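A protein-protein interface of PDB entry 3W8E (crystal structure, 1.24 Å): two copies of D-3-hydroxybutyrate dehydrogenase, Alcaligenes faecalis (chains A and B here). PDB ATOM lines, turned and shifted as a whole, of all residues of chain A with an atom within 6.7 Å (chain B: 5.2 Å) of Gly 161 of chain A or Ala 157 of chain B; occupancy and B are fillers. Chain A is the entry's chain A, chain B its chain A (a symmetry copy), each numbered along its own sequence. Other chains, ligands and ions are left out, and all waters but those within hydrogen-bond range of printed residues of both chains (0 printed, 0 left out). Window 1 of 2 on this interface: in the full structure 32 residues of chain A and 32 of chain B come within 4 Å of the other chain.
ND1 of His 160 of chain A sits close to O of Gly 145 of chain A (3.4 Å).
The backbone carbonyl oxygen (O) of Val 156 of chain A sits at hydrogen-bond distance from a ring nitrogen (ND1) of His 160 of chain A.
A ring nitrogen (ND1) of His 160 of chain B sits at hydrogen-bond distance from the backbone carbonyl oxygen of Val 156 of chain B (3.0 Å).
CG of Leu 115 of chain A touches CZ2 of Trp 107 of chain B (3.97 Å).
Ala 157 of chain A touches Gly 161 of chain B.
His 160 of chain A touches His 160 of chain B (O to CB, 3.2 Å).
CA of Gly 161 of chain A touches O of Ala 157 of chain B (3.4 Å).
N of Gly 161 of chain B touches N of Gly 161 of chain A, 3.997 Å away.
Val 156 of chain B touches Gly 164 of chain A (CG1 to O, 3.6 Å).
His 160 of chain B touches Gly 164 of chain A (CD2 to CA, 3.5 Å).
Leu 165 of chain A touches Ser 153 of chain B (CD1 to CB, 3.7 Å).
Ser 153 of chain B touches Val 168 of chain A.
Val 168 of chain A touches Val 156 of chain B (CG2 to CB, 3.7 Å).
Of the printed residues of chain B, Ala 157 of chain A touches Gly 161.
Lys 159 of chain A touches none of the printed residues of chain B.
Printed residues of chain B within 4 Å of Gly 161 of chain A: Ala 157 (3.4 Å) and Gly 161 (3.997 Å).
Printed residues of chain B within 4 Å of Leu 165 of chain A: Ser 153 (3.7 Å).
Printed residues of chain A within 4 Å of Trp 107 of chain B: Leu 115 (3.97 Å).
Of the printed residues of chain A, Ala 157 of chain B touches Gly 161.
Printed residues of chain A within 4 Å of His 160 of chain B: His 160 and Gly 164.
The nearest printed residue of chain A that does not touch Ser 153 of chain B is Gly 164 of chain A (5.7 Å).
Of the 14 printed residues of chain B, 6 touch a printed residue of chain A.
Hydrophobic or aromatic side chains of chain B that line the printed part of chain A: Trp 107, Val 156, Ala 157 and His 160.
Hydrophobic or aromatic side chains of chain A that line the printed part of chain B: Leu 115, Ala 157, His 160, Leu 165 and Val 168.
Among the printed residues, no Asp or Glu carboxylate lies within 4 Å of a Lys or Arg side-chain nitrogen of the other chain.
Ala 157 of chain A touches Gly 161 of chain B, and with the chains exchanged Gly 161 of chain A touches Ala 157 of chain B.
His 160 of chain B touches its own counterpart, His 160 of chain A.
Gly 161 of chain A touches its own counterpart, Gly 161 of chain B.
Positions printed for both chains: 115, 155, 156, 157, 158, 159, 160, 161 and 162.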
ATOM      1  N   ASN A 114     -19.411  13.843  17.142  1.00  0.00           N
ATOM      2  CA  ASN A 114     -20.202  13.338  18.275  1.00  0.00           C
ATOM      3  C   ASN A 114     -19.768  13.936  19.597  1.00  0.00           C
ATOM      4  O   ASN A 114     -20.570  13.867  20.541  1.00  0.00           O
ATOM      5  CB  ASN A 114     -20.125  11.792  18.338  1.00  0.00           C
ATOM      6  CG  ASN A 114     -20.708  11.099  17.149  1.00  0.00           C
ATOM      7  OD1 ASN A 114     -20.832  11.599  16.021  1.00  0.00           O
ATOM      8  ND2 ASN A 114     -21.085   9.820  17.338  1.00  0.00           N
ATOM      9  N   LEU A 115     -18.564  14.455  19.724  1.00  0.00           N
ATOM     10  CA  LEU A 115     -18.120  15.018  21.002  1.00  0.00           C
ATOM     11  C   LEU A 115     -17.785  16.491  20.815  1.00  0.00           C
ATOM     12  O   LEU A 115     -18.386  17.343  21.447  1.00  0.00           O
ATOM     13  CB  LEU A 115     -16.977  14.224  21.607  1.00  0.00           C
ATOM     14  CG  LEU A 115     -16.389  14.799  22.860  1.00  0.00           C
ATOM     15  CD1 LEU A 115     -17.436  14.996  23.963  1.00  0.00           C
ATOM     16  CD2 LEU A 115     -15.215  13.918  23.340  1.00  0.00           C
ATOM     17  N   GLY A 145     -23.133   6.002  26.159  1.00  0.00           N
ATOM     18  CA  GLY A 145     -22.586   7.023  27.002  1.00  0.00           C
ATOM     19  C   GLY A 145     -22.399   6.523  28.447  1.00  0.00           C
ATOM     20  O   GLY A 145     -21.750   7.181  29.232  1.00  0.00           O
ATOM     21  N   TYR A 155     -17.229   5.675  19.111  1.00  0.00           N
ATOM     22  CA  TYR A 155     -18.565   6.141  19.471  1.00  0.00           C
ATOM     23  C   TYR A 155     -18.834   6.100  20.989  1.00  0.00           C
ATOM     24  O   TYR A 155     -19.379   6.999  21.547  1.00  0.00           O
ATOM     25  CB  TYR A 155     -19.557   5.288  18.723  1.00  0.00           C
ATOM     26  CG  TYR A 155     -20.993   5.645  18.847  1.00  0.00           C
ATOM     27  CD1 TYR A 155     -21.816   5.116  19.848  1.00  0.00           C
ATOM     28  CD2 TYR A 155     -21.580   6.479  17.899  1.00  0.00           C
ATOM     29  CE1 TYR A 155     -23.193   5.410  19.897  1.00  0.00           C
ATOM     30  CE2 TYR A 155     -22.928   6.827  17.956  1.00  0.00           C
ATOM     31  CZ  TYR A 155     -23.745   6.204  18.944  1.00  0.00           C
ATOM     32  OH  TYR A 155     -25.073   6.496  19.028  1.00  0.00           O
ATOM     33  N   VAL A 156     -18.429   4.956  21.599  1.00  0.00           N
ATOM     34  CA  VAL A 156     -18.540   4.853  23.059  1.00  0.00           C
ATOM     35  C   VAL A 156     -17.733   5.897  23.738  1.00  0.00           C
ATOM     36  O   VAL A 156     -18.191   6.549  24.720  1.00  0.00           O
ATOM     37  CB  VAL A 156     -18.165   3.430  23.515  1.00  0.00           C
ATOM     38  CG1 VAL A 156     -18.157   3.349  25.050  1.00  0.00           C
ATOM     39  CG2 VAL A 156     -19.163   2.387  23.017  1.00  0.00           C
ATOM     40  N   ALA A 157     -16.485   6.094  23.302  1.00  0.00           N
ATOM     41  CA  ALA A 157     -15.709   7.163  23.879  1.00  0.00           C
ATOM     42  C   ALA A 157     -16.346   8.503  23.763  1.00  0.00           C
ATOM     43  O   ALA A 157     -16.441   9.303  24.717  1.00  0.00           O
ATOM     44  CB  ALA A 157     -14.265   7.164  23.321  1.00  0.00           C
ATOM     45  N   ALA A 158     -16.832   8.826  22.550  1.00  0.00           N
ATOM     46  CA  ALA A 158     -17.431  10.095  22.332  1.00  0.00           C
ATOM     47  C   ALA A 158     -18.677  10.326  23.228  1.00  0.00           C
ATOM     48  O   ALA A 158     -18.901  11.388  23.754  1.00  0.00           O
ATOM     49  CB  ALA A 158     -17.860  10.251  20.825  1.00  0.00           C
ATOM     50  N   LYS A 159     -19.532   9.275  23.248  1.00  0.00           N
ATOM     51  CA  LYS A 159     -20.806   9.407  23.975  1.00  0.00           C
ATOM     52  C   LYS A 159     -20.541   9.472  25.467  1.00  0.00           C
ATOM     53  O   LYS A 159     -21.233  10.212  26.180  1.00  0.00           O
ATOM     54  CB  LYS A 159     -21.761   8.260  23.639  1.00  0.00           C
ATOM     55  CG  LYS A 159     -22.263   8.291  22.240  1.00  0.00           C
ATOM     56  CD  LYS A 159     -23.038   9.550  21.867  1.00  0.00           C
ATOM     57  CE  LYS A 159     -23.720   9.414  20.523  1.00  0.00           C
ATOM     58  NZ  LYS A 159     -24.524  10.594  20.231  1.00  0.00           N
ATOM     59  N   HIS A 160     -19.588   8.693  25.969  1.00  0.00           N
ATOM     60  CA  HIS A 160     -19.175   8.898  27.382  1.00  0.00           C
ATOM     61  C   HIS A 160     -18.679  10.320  27.585  1.00  0.00           C
ATOM     62  O   HIS A 160     -19.046  10.996  28.599  1.00  0.00           O
ATOM     63  CB  HIS A 160     -18.048   7.955  27.820  1.00  0.00           C
ATOM     64  CG  HIS A 160     -18.534   6.595  28.235  1.00  0.00           C
ATOM     65  ND1 HIS A 160     -19.234   5.723  27.423  1.00  0.00           N
ATOM     66  CD2 HIS A 160     -18.417   5.971  29.457  1.00  0.00           C
ATOM     67  CE1 HIS A 160     -19.537   4.612  28.128  1.00  0.00           C
ATOM     68  NE2 HIS A 160     -19.059   4.746  29.347  1.00  0.00           N
ATOM     69  N   GLY A 161     -17.891  10.851  26.645  1.00  0.00           N
ATOM     70  CA  GLY A 161     -17.497  12.255  26.705  1.00  0.00           C
ATOM     71  C   GLY A 161     -18.627  13.249  26.779  1.00  0.00           C
ATOM     72  O   GLY A 161     -18.568  14.198  27.519  1.00  0.00           O
ATOM     73  N   VAL A 162     -19.679  12.994  25.969  1.00  0.00           N
ATOM     74  CA  VAL A 162     -20.858  13.860  25.971  1.00  0.00           C
ATOM     75  C   VAL A 162     -21.512  13.857  27.344  1.00  0.00           C
ATOM     76  O   VAL A 162     -21.939  14.856  27.850  1.00  0.00           O
ATOM     77  CB  VAL A 162     -21.838  13.471  24.893  1.00  0.00           C
ATOM     78  CG1 VAL A 162     -23.170  14.212  25.077  1.00  0.00           C
ATOM     79  CG2 VAL A 162     -21.248  13.747  23.531  1.00  0.00           C
ATOM     80  N   VAL A 163     -21.613  12.652  27.931  1.00  0.00           N
ATOM     81  CA  VAL A 163     -22.154  12.637  29.328  1.00  0.00           C
ATOM     82  C   VAL A 163     -21.334  13.404  30.291  1.00  0.00           C
ATOM     83  O   VAL A 163     -21.912  14.199  31.096  1.00  0.00           O
ATOM     84  CB  VAL A 163     -22.317  11.135  29.700  1.00  0.00           C
ATOM     85  CG1 VAL A 163     -22.625  10.947  31.188  1.00  0.00           C
ATOM     86  CG2 VAL A 163     -23.396  10.484  28.869  1.00  0.00           C
ATOM     87  N   GLY A 164     -20.026  13.331  30.218  1.00  0.00           N
ATOM     88  CA  GLY A 164     -19.192  14.169  31.069  1.00  0.00           C
ATOM     89  C   GLY A 164     -19.358  15.641  30.799  1.00  0.00           C
ATOM     90  O   GLY A 164     -19.449  16.446  31.766  1.00  0.00           O
ATOM     91  N   LEU A 165     -19.377  16.012  29.530  1.00  0.00           N
ATOM     92  CA  LEU A 165     -19.517  17.397  29.191  1.00  0.00           C
ATOM     93  C   LEU A 165     -20.841  17.947  29.661  1.00  0.00           C
ATOM     94  O   LEU A 165     -20.921  19.103  30.089  1.00  0.00           O
ATOM     95  CB  LEU A 165     -19.409  17.515  27.647  1.00  0.00           C
ATOM     96  CG  LEU A 165     -19.510  18.894  27.085  1.00  0.00           C
ATOM     97  CD1 LEU A 165     -18.440  19.850  27.636  1.00  0.00           C
ATOM     98  CD2 LEU A 165     -19.442  18.760  25.535  1.00  0.00           C
ATOM     99  N   THR A 166     -21.887  17.142  29.573  1.00  0.00           N
ATOM    100  CA  THR A 166     -23.208  17.555  30.040  1.00  0.00           C
ATOM    101  C   THR A 166     -23.130  17.943  31.532  1.00  0.00           C
ATOM    102  O   THR A 166     -23.751  18.927  31.966  1.00  0.00           O
ATOM    103  CB  THR A 166     -24.176  16.374  29.875  1.00  0.00           C
ATOM    104  OG1 THR A 166     -24.327  16.112  28.426  1.00  0.00           O
ATOM    105  CG2 THR A 166     -25.530  16.628  30.422  1.00  0.00           C
ATOM    106  N   VAL A 168     -20.499  18.919  33.302  1.00  0.00           N
ATOM    107  CA  VAL A 168     -19.784  20.134  33.465  1.00  0.00           C
ATOM    108  C   VAL A 168     -20.611  21.364  33.119  1.00  0.00           C
ATOM    109  O   VAL A 168     -20.686  22.362  33.853  1.00  0.00           O
ATOM    110  CB  VAL A 168     -18.424  20.164  32.662  1.00  0.00           C
ATOM    111  CG1 VAL A 168     -17.790  21.584  32.776  1.00  0.00           C
ATOM    112  CG2 VAL A 168     -17.513  19.158  33.123  1.00  0.00           C
ATOM    113  N   TRP B 107      -8.961  22.731  24.217  1.00  0.00           N
ATOM    114  CA  TRP B 107      -9.897  21.576  23.976  1.00  0.00           C
ATOM    115  C   TRP B 107      -9.234  20.561  23.110  1.00  0.00           C
ATOM    116  O   TRP B 107      -9.122  19.343  23.437  1.00  0.00           O
ATOM    117  CB  TRP B 107     -11.213  22.068  23.379  1.00  0.00           C
ATOM    118  CG  TRP B 107     -12.090  20.939  22.901  1.00  0.00           C
ATOM    119  CD1 TRP B 107     -12.064  20.351  21.698  1.00  0.00           C
ATOM    120  CD2 TRP B 107     -13.065  20.225  23.674  1.00  0.00           C
ATOM    121  NE1 TRP B 107     -13.009  19.303  21.625  1.00  0.00           N
ATOM    122  CE2 TRP B 107     -13.565  19.209  22.886  1.00  0.00           C
ATOM    123  CE3 TRP B 107     -13.556  20.382  24.986  1.00  0.00           C
ATOM    124  CZ2 TRP B 107     -14.537  18.281  23.335  1.00  0.00           C
ATOM    125  CZ3 TRP B 107     -14.583  19.421  25.350  1.00  0.00           C
ATOM    126  CH2 TRP B 107     -14.960  18.427  24.570  1.00  0.00           C
ATOM    127  N   ILE B 111      -8.145  16.720  24.348  1.00  0.00           N
ATOM    128  CA  ILE B 111      -8.760  15.555  23.707  1.00  0.00           C
ATOM    129  C   ILE B 111      -7.655  14.716  23.053  1.00  0.00           C
ATOM    130  O   ILE B 111      -7.627  13.467  23.155  1.00  0.00           O
ATOM    131  CB  ILE B 111      -9.801  15.998  22.724  1.00  0.00           C
ATOM    132  CG1 ILE B 111     -11.025  16.657  23.421  1.00  0.00           C
ATOM    133  CG2 ILE B 111     -10.305  14.802  21.779  1.00  0.00           C
ATOM    134  CD1 ILE B 111     -11.752  15.797  24.477  1.00  0.00           C
ATOM    135  N   LEU B 115      -7.343  11.617  25.544  1.00  0.00           N
ATOM    136  CA  LEU B 115      -8.295  10.625  25.037  1.00  0.00           C
ATOM    137  C   LEU B 115      -7.702   9.934  23.817  1.00  0.00           C
ATOM    138  O   LEU B 115      -7.521   8.729  23.821  1.00  0.00           O
ATOM    139  CB  LEU B 115      -9.660  11.232  24.768  1.00  0.00           C
ATOM    140  CG  LEU B 115     -10.660  10.309  24.140  1.00  0.00           C
ATOM    141  CD1 LEU B 115     -10.886   9.039  24.969  1.00  0.00           C
ATOM    142  CD2 LEU B 115     -11.982  11.066  23.885  1.00  0.00           C
ATOM    143  N   LYS B 152     -13.762  22.399  33.851  1.00  0.00           N
ATOM    144  CA  LYS B 152     -12.889  21.322  33.385  1.00  0.00           C
ATOM    145  C   LYS B 152     -13.564  20.572  32.280  1.00  0.00           C
ATOM    146  O   LYS B 152     -13.469  19.357  32.137  1.00  0.00           O
ATOM    147  CB  LYS B 152     -12.506  20.382  34.523  1.00  0.00           C
ATOM    148  CG  LYS B 152     -11.542  21.091  35.493  1.00  0.00           C
ATOM    149  CD  LYS B 152     -11.114  20.132  36.667  1.00  0.00           C
ATOM    150  CE  LYS B 152     -10.037  20.867  37.450  1.00  0.00           C
ATOM    151  NZ  LYS B 152      -9.628  20.062  38.623  1.00  0.00           N
ATOM    152  N   SER B 153     -14.287  21.304  31.393  1.00  0.00           N
ATOM    153  CA  SER B 153     -15.044  20.619  30.313  1.00  0.00           C
ATOM    154  C   SER B 153     -14.194  19.657  29.507  1.00  0.00           C
ATOM    155  O   SER B 153     -14.583  18.473  29.310  1.00  0.00           O
ATOM    156  CB  SER B 153     -15.676  21.608  29.409  1.00  0.00           C
ATOM    157  OG  SER B 153     -14.767  22.561  28.863  1.00  0.00           O
ATOM    158  N   ALA B 154     -13.017  20.094  28.975  1.00  0.00           N
ATOM    159  CA  ALA B 154     -12.305  19.216  28.092  1.00  0.00           C
ATOM    160  C   ALA B 154     -11.786  17.965  28.843  1.00  0.00           C
ATOM    161  O   ALA B 154     -11.750  16.878  28.337  1.00  0.00           O
ATOM    162  CB  ALA B 154     -11.066  19.946  27.477  1.00  0.00           C
ATOM    163  N   TYR B 155     -11.239  18.237  30.044  1.00  0.00           N
ATOM    164  CA  TYR B 155     -10.645  17.144  30.809  1.00  0.00           C
ATOM    165  C   TYR B 155     -11.676  16.090  31.261  1.00  0.00           C
ATOM    166  O   TYR B 155     -11.446  14.924  31.182  1.00  0.00           O
ATOM    167  CB  TYR B 155      -9.941  17.755  31.993  1.00  0.00           C
ATOM    168  CG  TYR B 155      -9.164  16.842  32.869  1.00  0.00           C
ATOM    169  CD1 TYR B 155      -9.731  16.199  33.976  1.00  0.00           C
ATOM    170  CD2 TYR B 155      -7.802  16.661  32.642  1.00  0.00           C
ATOM    171  CE1 TYR B 155      -8.954  15.399  34.838  1.00  0.00           C
ATOM    172  CE2 TYR B 155      -7.023  15.833  33.448  1.00  0.00           C
ATOM    173  CZ  TYR B 155      -7.622  15.263  34.608  1.00  0.00           C
ATOM    174  OH  TYR B 155      -6.897  14.462  35.439  1.00  0.00           O
ATOM    175  N   VAL B 156     -12.821  16.609  31.775  1.00  0.00           N
ATOM    176  CA  VAL B 156     -13.913  15.699  32.139  1.00  0.00           C
ATOM    177  C   VAL B 156     -14.392  14.930  30.963  1.00  0.00           C
ATOM    178  O   VAL B 156     -14.631  13.691  31.038  1.00  0.00           O
ATOM    179  CB  VAL B 156     -15.043  16.483  32.830  1.00  0.00           C
ATOM    180  CG1 VAL B 156     -16.242  15.560  33.101  1.00  0.00           C
ATOM    181  CG2 VAL B 156     -14.605  17.055  34.176  1.00  0.00           C
ATOM    182  N   ALA B 157     -14.605  15.606  29.830  1.00  0.00           N
ATOM    183  CA  ALA B 157     -14.981  14.874  28.646  1.00  0.00           C
ATOM    184  C   ALA B 157     -14.011  13.816  28.256  1.00  0.00           C
ATOM    185  O   ALA B 157     -14.348  12.651  27.958  1.00  0.00           O
ATOM    186  CB  ALA B 157     -15.283  15.837  27.471  1.00  0.00           C
ATOM    187  N   ALA B 158     -12.714  14.176  28.239  1.00  0.00           N
ATOM    188  CA  ALA B 158     -11.715  13.245  27.851  1.00  0.00           C
ATOM    189  C   ALA B 158     -11.670  12.000  28.777  1.00  0.00           C
ATOM    190  O   ALA B 158     -11.509  10.885  28.347  1.00  0.00           O
ATOM    191  CB  ALA B 158     -10.295  13.924  27.854  1.00  0.00           C
ATOM    192  N   LYS B 159     -11.699  12.306  30.097  1.00  0.00           N
ATOM    193  CA  LYS B 159     -11.555  11.222  31.083  1.00  0.00           C
ATOM    194  C   LYS B 159     -12.788  10.340  31.060  1.00  0.00           C
ATOM    195  O   LYS B 159     -12.669   9.117  31.217  1.00  0.00           O
ATOM    196  CB  LYS B 159     -11.304  11.776  32.487  1.00  0.00           C
ATOM    197  CG  LYS B 159      -9.981  12.437  32.641  1.00  0.00           C
ATOM    198  CD  LYS B 159      -8.781  11.536  32.369  1.00  0.00           C
ATOM    199  CE  LYS B 159      -7.480  12.194  32.774  1.00  0.00           C
ATOM    200  NZ  LYS B 159      -6.360  11.280  32.587  1.00  0.00           N
ATOM    201  N   HIS B 160     -13.972  10.923  30.911  1.00  0.00           N
ATOM    202  CA  HIS B 160     -15.163  10.063  30.675  1.00  0.00           C
ATOM    203  C   HIS B 160     -14.967   9.225  29.423  1.00  0.00           C
ATOM    204  O   HIS B 160     -15.266   7.988  29.419  1.00  0.00           O
ATOM    205  CB  HIS B 160     -16.456  10.867  30.489  1.00  0.00           C
ATOM    206  CG  HIS B 160     -17.097  11.276  31.784  1.00  0.00           C
ATOM    207  ND1 HIS B 160     -16.499  12.062  32.751  1.00  0.00           N
ATOM    208  CD2 HIS B 160     -18.342  10.948  32.273  1.00  0.00           C
ATOM    209  CE1 HIS B 160     -17.346  12.202  33.792  1.00  0.00           C
ATOM    210  NE2 HIS B 160     -18.452  11.539  33.524  1.00  0.00           N
ATOM    211  N   GLY B 161     -14.428   9.813  28.350  1.00  0.00           N
ATOM    212  CA  GLY B 161     -14.081   9.034  27.166  1.00  0.00           C
ATOM    213  C   GLY B 161     -13.152   7.870  27.398  1.00  0.00           C
ATOM    214  O   GLY B 161     -13.343   6.811  26.856  1.00  0.00           O
ATOM    215  N   VAL B 162     -12.119   8.109  28.237  1.00  0.00           N
ATOM    216  CA  VAL B 162     -11.165   7.053  28.576  1.00  0.00           C
ATOM    217  C   VAL B 162     -11.877   5.905  29.275  1.00  0.00           C
ATOM    218  O   VAL B 162     -11.626   4.757  29.035  1.00  0.00           O
ATOM    219  CB  VAL B 162     -10.022   7.580  29.407  1.00  0.00           C
ATOM    220  CG1 VAL B 162      -9.182   6.424  29.968  1.00  0.00           C
ATOM    221  CG2 VAL B 162      -9.173   8.518  28.585  1.00  0.00           C
